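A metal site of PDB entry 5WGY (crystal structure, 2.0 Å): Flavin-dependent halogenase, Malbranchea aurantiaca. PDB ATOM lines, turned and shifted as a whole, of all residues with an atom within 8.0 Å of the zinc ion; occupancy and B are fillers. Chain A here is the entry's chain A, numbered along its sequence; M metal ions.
The zinc ion is bound by the side-chain sulfur (SG) of Cys 613, the side-chain sulfur (SG) of Cys 600, the side-chain sulfur (SG) of Cys 616 and the side-chain sulfur (SG) of Cys 597.
The backbone NH (N) of Ser 615 lies close to the side-chain sulfur (SG) of Cys 613, at 3.3 Å.
The backbone carbonyl oxygen (O) of Leu 618 sits at hydrogen-bond distance from the backbone NH (N) of Cys 613 (2.9 Å).
N of Ala 602 lies close to SG of Cys 600 (3.4 Å).
SG of Cys 616 lies close to N of Leu 618 (3.4 Å).
The side-chain sulfur of Cys 597 sits close to the backbone NH of Gly 599 (3.4 Å).
N of Cys 597 lies within hydrogen-bond range of O of Ala 602, 2.8 Å away.
Within 4 Å of the zinc ion: Cys 597, Cys 600, Cys 613 and Cys 616.
The nearest printed residue that does not touch the zinc ion is Gly 617 (4.7 Å).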
ATOM      1  N   ARG A 268      -2.195   1.769  34.156  1.00  0.00           N
ATOM      2  CA  ARG A 268      -3.480   1.642  33.462  1.00  0.00           C
ATOM      3  C   ARG A 268      -3.339   2.182  32.029  1.00  0.00           C
ATOM      4  O   ARG A 268      -2.963   3.336  31.824  1.00  0.00           O
ATOM      5  CB  ARG A 268      -4.553   2.433  34.222  1.00  0.00           C
ATOM      6  CG  ARG A 268      -5.967   2.253  33.655  1.00  0.00           C
ATOM      7  CD  ARG A 268      -6.973   3.281  34.212  1.00  0.00           C
ATOM      8  NE  ARG A 268      -8.018   3.493  33.220  1.00  0.00           N
ATOM      9  CZ  ARG A 268      -9.239   2.963  33.272  1.00  0.00           C
ATOM     10  NH1 ARG A 268      -9.607   2.202  34.318  1.00  0.00           N
ATOM     11  NH2 ARG A 268     -10.085   3.210  32.273  1.00  0.00           N
ATOM     12  N   SER A 302     -13.961   9.691  19.662  1.00  0.00           N
ATOM     13  CA  SER A 302     -13.317   9.091  20.816  1.00  0.00           C
ATOM     14  C   SER A 302     -12.608   7.797  20.418  1.00  0.00           C
ATOM     15  O   SER A 302     -12.797   7.269  19.320  1.00  0.00           O
ATOM     16  CB  SER A 302     -14.334   8.798  21.921  1.00  0.00           C
ATOM     17  OG  SER A 302     -15.244   7.789  21.537  1.00  0.00           O
ATOM     18  N   GLU A 304     -13.194   4.815  21.459  1.00  0.00           N
ATOM     19  CA  GLU A 304     -14.151   3.755  21.138  1.00  0.00           C
ATOM     20  C   GLU A 304     -14.832   4.001  19.806  1.00  0.00           C
ATOM     21  O   GLU A 304     -15.181   3.043  19.117  1.00  0.00           O
ATOM     22  CB  GLU A 304     -15.189   3.621  22.255  1.00  0.00           C
ATOM     23  CG  GLU A 304     -14.632   2.963  23.543  1.00  0.00           C
ATOM     24  CD  GLU A 304     -15.647   2.956  24.702  1.00  0.00           C
ATOM     25  OE1 GLU A 304     -16.877   3.071  24.446  1.00  0.00           O
ATOM     26  OE2 GLU A 304     -15.207   2.838  25.853  1.00  0.00           O
ATOM     27  N   TRP A 316      -9.533  -1.758  28.073  1.00  0.00           N
ATOM     28  CA  TRP A 316      -8.719  -1.201  29.150  1.00  0.00           C
ATOM     29  C   TRP A 316      -8.042  -2.348  29.917  1.00  0.00           C
ATOM     30  O   TRP A 316      -8.699  -3.314  30.308  1.00  0.00           O
ATOM     31  CB  TRP A 316      -9.590  -0.355  30.083  1.00  0.00           C
ATOM     32  CG  TRP A 316      -9.847   1.008  29.512  1.00  0.00           C
ATOM     33  CD1 TRP A 316     -11.003   1.460  28.939  1.00  0.00           C
ATOM     34  CD2 TRP A 316      -8.910   2.085  29.441  1.00  0.00           C
ATOM     35  NE1 TRP A 316     -10.835   2.759  28.500  1.00  0.00           N
ATOM     36  CE2 TRP A 316      -9.568   3.172  28.804  1.00  0.00           C
ATOM     37  CE3 TRP A 316      -7.579   2.241  29.845  1.00  0.00           C
ATOM     38  CZ2 TRP A 316      -8.939   4.404  28.582  1.00  0.00           C
ATOM     39  CZ3 TRP A 316      -6.959   3.475  29.618  1.00  0.00           C
ATOM     40  CH2 TRP A 316      -7.637   4.526  28.979  1.00  0.00           C
ATOM     41  N   ARG A 595     -10.131  13.659  36.315  1.00  0.00           N
ATOM     42  CA  ARG A 595     -11.330  12.984  36.822  1.00  0.00           C
ATOM     43  C   ARG A 595     -11.549  11.726  35.997  1.00  0.00           C
ATOM     44  O   ARG A 595     -11.026  11.596  34.880  1.00  0.00           O
ATOM     45  CB  ARG A 595     -12.585  13.881  36.728  1.00  0.00           C
ATOM     46  CG  ARG A 595     -13.036  14.075  35.289  1.00  0.00           C
ATOM     47  CD  ARG A 595     -14.312  14.920  35.142  1.00  0.00           C
ATOM     48  NE  ARG A 595     -14.760  14.930  33.732  1.00  0.00           N
ATOM     49  CZ  ARG A 595     -15.703  14.121  33.251  1.00  0.00           C
ATOM     50  NH1 ARG A 595     -16.318  13.253  34.072  1.00  0.00           N
ATOM     51  NH2 ARG A 595     -16.032  14.180  31.950  1.00  0.00           N
ATOM     52  N   GLN A 596     -12.320  10.790  36.552  1.00  0.00           N
ATOM     53  CA  GLN A 596     -12.709   9.554  35.860  1.00  0.00           C
ATOM     54  C   GLN A 596     -14.039   9.734  35.145  1.00  0.00           C
ATOM     55  O   GLN A 596     -15.005  10.215  35.741  1.00  0.00           O
ATOM     56  CB  GLN A 596     -12.825   8.396  36.842  1.00  0.00           C
ATOM     57  CG  GLN A 596     -11.703   7.405  36.809  1.00  0.00           C
ATOM     58  CD  GLN A 596     -11.999   6.188  37.640  1.00  0.00           C
ATOM     59  OE1 GLN A 596     -12.334   6.297  38.808  1.00  0.00           O
ATOM     60  NE2 GLN A 596     -11.890   5.010  37.028  1.00  0.00           N
ATOM     61  N   CYS A 597     -14.084   9.351  33.872  1.00  0.00           N
ATOM     62  CA  CYS A 597     -15.361   9.301  33.181  1.00  0.00           C
ATOM     63  C   CYS A 597     -16.302   8.392  33.960  1.00  0.00           C
ATOM     64  O   CYS A 597     -15.927   7.285  34.351  1.00  0.00           O
ATOM     65  CB  CYS A 597     -15.175   8.785  31.757  1.00  0.00           C
ATOM     66  SG  CYS A 597     -16.728   8.722  30.855  1.00  0.00           S
ATOM     67  N   SER A 598     -17.516   8.872  34.232  1.00  0.00           N
ATOM     68  CA  SER A 598     -18.446   8.062  35.017  1.00  0.00           C
ATOM     69  C   SER A 598     -19.052   6.945  34.182  1.00  0.00           C
ATOM     70  O   SER A 598     -19.613   5.990  34.748  1.00  0.00           O
ATOM     71  CB  SER A 598     -19.552   8.926  35.635  1.00  0.00           C
ATOM     72  OG  SER A 598     -20.141   9.796  34.669  1.00  0.00           O
ATOM     73  N   GLY A 599     -18.940   7.032  32.856  1.00  0.00           N
ATOM     74  CA  GLY A 599     -19.467   6.030  31.951  1.00  0.00           C
ATOM     75  C   GLY A 599     -18.516   4.890  31.660  1.00  0.00           C
ATOM     76  O   GLY A 599     -18.896   3.709  31.770  1.00  0.00           O
ATOM     77  N   CYS A 600     -17.261   5.201  31.301  1.00  0.00           N
ATOM     78  CA  CYS A 600     -16.329   4.160  30.897  1.00  0.00           C
ATOM     79  C   CYS A 600     -15.139   3.964  31.846  1.00  0.00           C
ATOM     80  O   CYS A 600     -14.413   2.981  31.684  1.00  0.00           O
ATOM     81  CB  CYS A 600     -15.813   4.473  29.474  1.00  0.00           C
ATOM     82  SG  CYS A 600     -14.506   5.739  29.439  1.00  0.00           S
ATOM     83  N   GLY A 601     -14.937   4.850  32.839  1.00  0.00           N
ATOM     84  CA  GLY A 601     -13.830   4.721  33.781  1.00  0.00           C
ATOM     85  C   GLY A 601     -12.518   5.359  33.350  1.00  0.00           C
ATOM     86  O   GLY A 601     -11.590   5.433  34.184  1.00  0.00           O
ATOM     87  N   ALA A 602     -12.398   5.831  32.117  1.00  0.00           N
ATOM     88  CA  ALA A 602     -11.125   6.373  31.644  1.00  0.00           C
ATOM     89  C   ALA A 602     -10.782   7.665  32.385  1.00  0.00           C
ATOM     90  O   ALA A 602     -11.658   8.498  32.663  1.00  0.00           O
ATOM     91  CB  ALA A 602     -11.161   6.639  30.139  1.00  0.00           C
ATOM     92  N   TRP A 603      -9.494   7.861  32.670  1.00  0.00           N
ATOM     93  CA  TRP A 603      -9.049   9.109  33.261  1.00  0.00           C
ATOM     94  C   TRP A 603      -8.925  10.212  32.214  1.00  0.00           C
ATOM     95  O   TRP A 603      -8.412   9.990  31.113  1.00  0.00           O
ATOM     96  CB  TRP A 603      -7.732   8.900  34.008  1.00  0.00           C
ATOM     97  CG  TRP A 603      -7.990   8.119  35.297  1.00  0.00           C
ATOM     98  CD1 TRP A 603      -7.995   6.761  35.465  1.00  0.00           C
ATOM     99  CD2 TRP A 603      -8.323   8.687  36.566  1.00  0.00           C
ATOM    100  NE1 TRP A 603      -8.282   6.441  36.783  1.00  0.00           N
ATOM    101  CE2 TRP A 603      -8.495   7.609  37.476  1.00  0.00           C
ATOM    102  CE3 TRP A 603      -8.515  10.004  37.032  1.00  0.00           C
ATOM    103  CZ2 TRP A 603      -8.840   7.809  38.819  1.00  0.00           C
ATOM    104  CZ3 TRP A 603      -8.857  10.199  38.367  1.00  0.00           C
ATOM    105  CH2 TRP A 603      -9.015   9.106  39.243  1.00  0.00           C
ATOM    106  N   LEU A 604      -9.415  11.403  32.584  1.00  0.00           N
ATOM    107  CA  LEU A 604      -9.523  12.569  31.720  1.00  0.00           C
ATOM    108  C   LEU A 604      -8.804  13.765  32.340  1.00  0.00           C
ATOM    109  O   LEU A 604      -8.753  13.905  33.565  1.00  0.00           O
ATOM    110  CB  LEU A 604     -10.998  12.970  31.501  1.00  0.00           C
ATOM    111  CG  LEU A 604     -11.972  11.853  31.118  1.00  0.00           C
ATOM    112  CD1 LEU A 604     -13.458  12.303  31.119  1.00  0.00           C
ATOM    113  CD2 LEU A 604     -11.551  11.281  29.769  1.00  0.00           C
ATOM    114  N   LYS A 612     -16.286  16.408  26.406  1.00  0.00           N
ATOM    115  CA  LYS A 612     -16.617  14.995  26.304  1.00  0.00           C
ATOM    116  C   LYS A 612     -15.399  14.143  26.644  1.00  0.00           C
ATOM    117  O   LYS A 612     -14.253  14.514  26.365  1.00  0.00           O
ATOM    118  CB  LYS A 612     -17.147  14.638  24.905  1.00  0.00           C
ATOM    119  CG  LYS A 612     -16.072  14.624  23.839  1.00  0.00           C
ATOM    120  CD  LYS A 612     -16.537  13.923  22.558  1.00  0.00           C
ATOM    121  CE  LYS A 612     -15.336  13.519  21.691  1.00  0.00           C
ATOM    122  NZ  LYS A 612     -15.703  13.313  20.239  1.00  0.00           N
ATOM    123  N   CYS A 613     -15.672  13.002  27.272  1.00  0.00           N
ATOM    124  CA  CYS A 613     -14.650  11.972  27.452  1.00  0.00           C
ATOM    125  C   CYS A 613     -13.988  11.660  26.112  1.00  0.00           C
ATOM    126  O   CYS A 613     -14.684  11.423  25.108  1.00  0.00           O
ATOM    127  CB  CYS A 613     -15.273  10.712  28.043  1.00  0.00           C
ATOM    128  SG  CYS A 613     -14.165   9.276  28.202  1.00  0.00           S
ATOM    129  N   HIS A 614     -12.652  11.705  26.076  1.00  0.00           N
ATOM    130  CA  HIS A 614     -11.925  11.439  24.835  1.00  0.00           C
ATOM    131  C   HIS A 614     -11.906   9.953  24.497  1.00  0.00           C
ATOM    132  O   HIS A 614     -11.487   9.576  23.385  1.00  0.00           O
ATOM    133  CB  HIS A 614     -10.460  11.946  24.904  1.00  0.00           C
ATOM    134  CG  HIS A 614      -9.606  11.174  25.860  1.00  0.00           C
ATOM    135  ND1 HIS A 614      -9.403  11.567  27.169  1.00  0.00           N
ATOM    136  CD2 HIS A 614      -8.931  10.012  25.703  1.00  0.00           C
ATOM    137  CE1 HIS A 614      -8.626  10.678  27.772  1.00  0.00           C
ATOM    138  NE2 HIS A 614      -8.331   9.727  26.904  1.00  0.00           N
ATOM    139  N   SER A 615     -12.324   9.110  25.421  1.00  0.00           N
ATOM    140  CA  SER A 615     -12.181   7.663  25.243  1.00  0.00           C
ATOM    141  C   SER A 615     -13.477   7.001  24.821  1.00  0.00           C
ATOM    142  O   SER A 615     -13.459   6.140  23.929  1.00  0.00           O
ATOM    143  CB  SER A 615     -11.681   7.033  26.542  1.00  0.00           C
ATOM    144  OG  SER A 615     -11.326   5.675  26.361  1.00  0.00           O
ATOM    145  N   CYS A 616     -14.606   7.394  25.416  1.00  0.00           N
ATOM    146  CA  CYS A 616     -15.908   6.871  25.033  1.00  0.00           C
ATOM    147  C   CYS A 616     -16.850   7.936  24.480  1.00  0.00           C
ATOM    148  O   CYS A 616     -17.929   7.575  23.980  1.00  0.00           O
ATOM    149  CB  CYS A 616     -16.571   6.169  26.227  1.00  0.00           C
ATOM    150  SG  CYS A 616     -17.497   7.244  27.359  1.00  0.00           S
ATOM    151  N   GLY A 617     -16.494   9.221  24.535  1.00  0.00           N
ATOM    152  CA  GLY A 617     -17.314  10.262  23.961  1.00  0.00           C
ATOM    153  C   GLY A 617     -18.446  10.762  24.834  1.00  0.00           C
ATOM    154  O   GLY A 617     -19.123  11.719  24.451  1.00  0.00           O
ATOM    155  N   LEU A 618     -18.679  10.144  25.985  1.00  0.00           N
ATOM    156  CA  LEU A 618     -19.784  10.589  26.824  1.00  0.00           C
ATOM    157  C   LEU A 618     -19.559  12.018  27.287  1.00  0.00           C
ATOM    158  O   LEU A 618     -18.492  12.356  27.841  1.00  0.00           O
ATOM    159  CB  LEU A 618     -19.957   9.669  28.036  1.00  0.00           C
ATOM    160  CG  LEU A 618     -20.840  10.148  29.196  1.00  0.00           C
ATOM    161  CD1 LEU A 618     -22.334  10.206  28.860  1.00  0.00           C
ATOM    162  CD2 LEU A 618     -20.599   9.238  30.358  1.00  0.00           C
ATOM    163  N   LEU A 619     -20.536  12.862  27.037  1.00  0.00           N
ATOM    164  CA  LEU A 619     -20.439  14.261  27.440  1.00  0.00           C
ATOM    165  C   LEU A 619     -20.322  14.313  28.957  1.00  0.00           C
ATOM    166  O   LEU A 619     -21.211  13.846  29.666  1.00  0.00           O
ATOM    167  CB  LEU A 619     -21.659  15.039  26.958  1.00  0.00           C
ATOM    168  CG  LEU A 619     -21.531  16.562  26.950  1.00  0.00           C
ATOM    169  CD1 LEU A 619     -20.406  16.997  26.021  1.00  0.00           C
ATOM    170  CD2 LEU A 619     -22.855  17.192  26.543  1.00  0.00           C
ATOM    171  N   GLY A 620     -19.179  14.802  29.446  1.00  0.00           N
ATOM    172  CA  GLY A 620     -19.071  15.149  30.844  1.00  0.00           C
ATOM    173  C   GLY A 620     -20.314  15.941  31.135  1.00  0.00           C
ATOM    174  O   GLY A 620     -20.655  16.824  30.345  1.00  0.00           O
HETATM  175 ZN    ZN M   1     -15.731   7.722  28.904  1.00  0.00          ZN
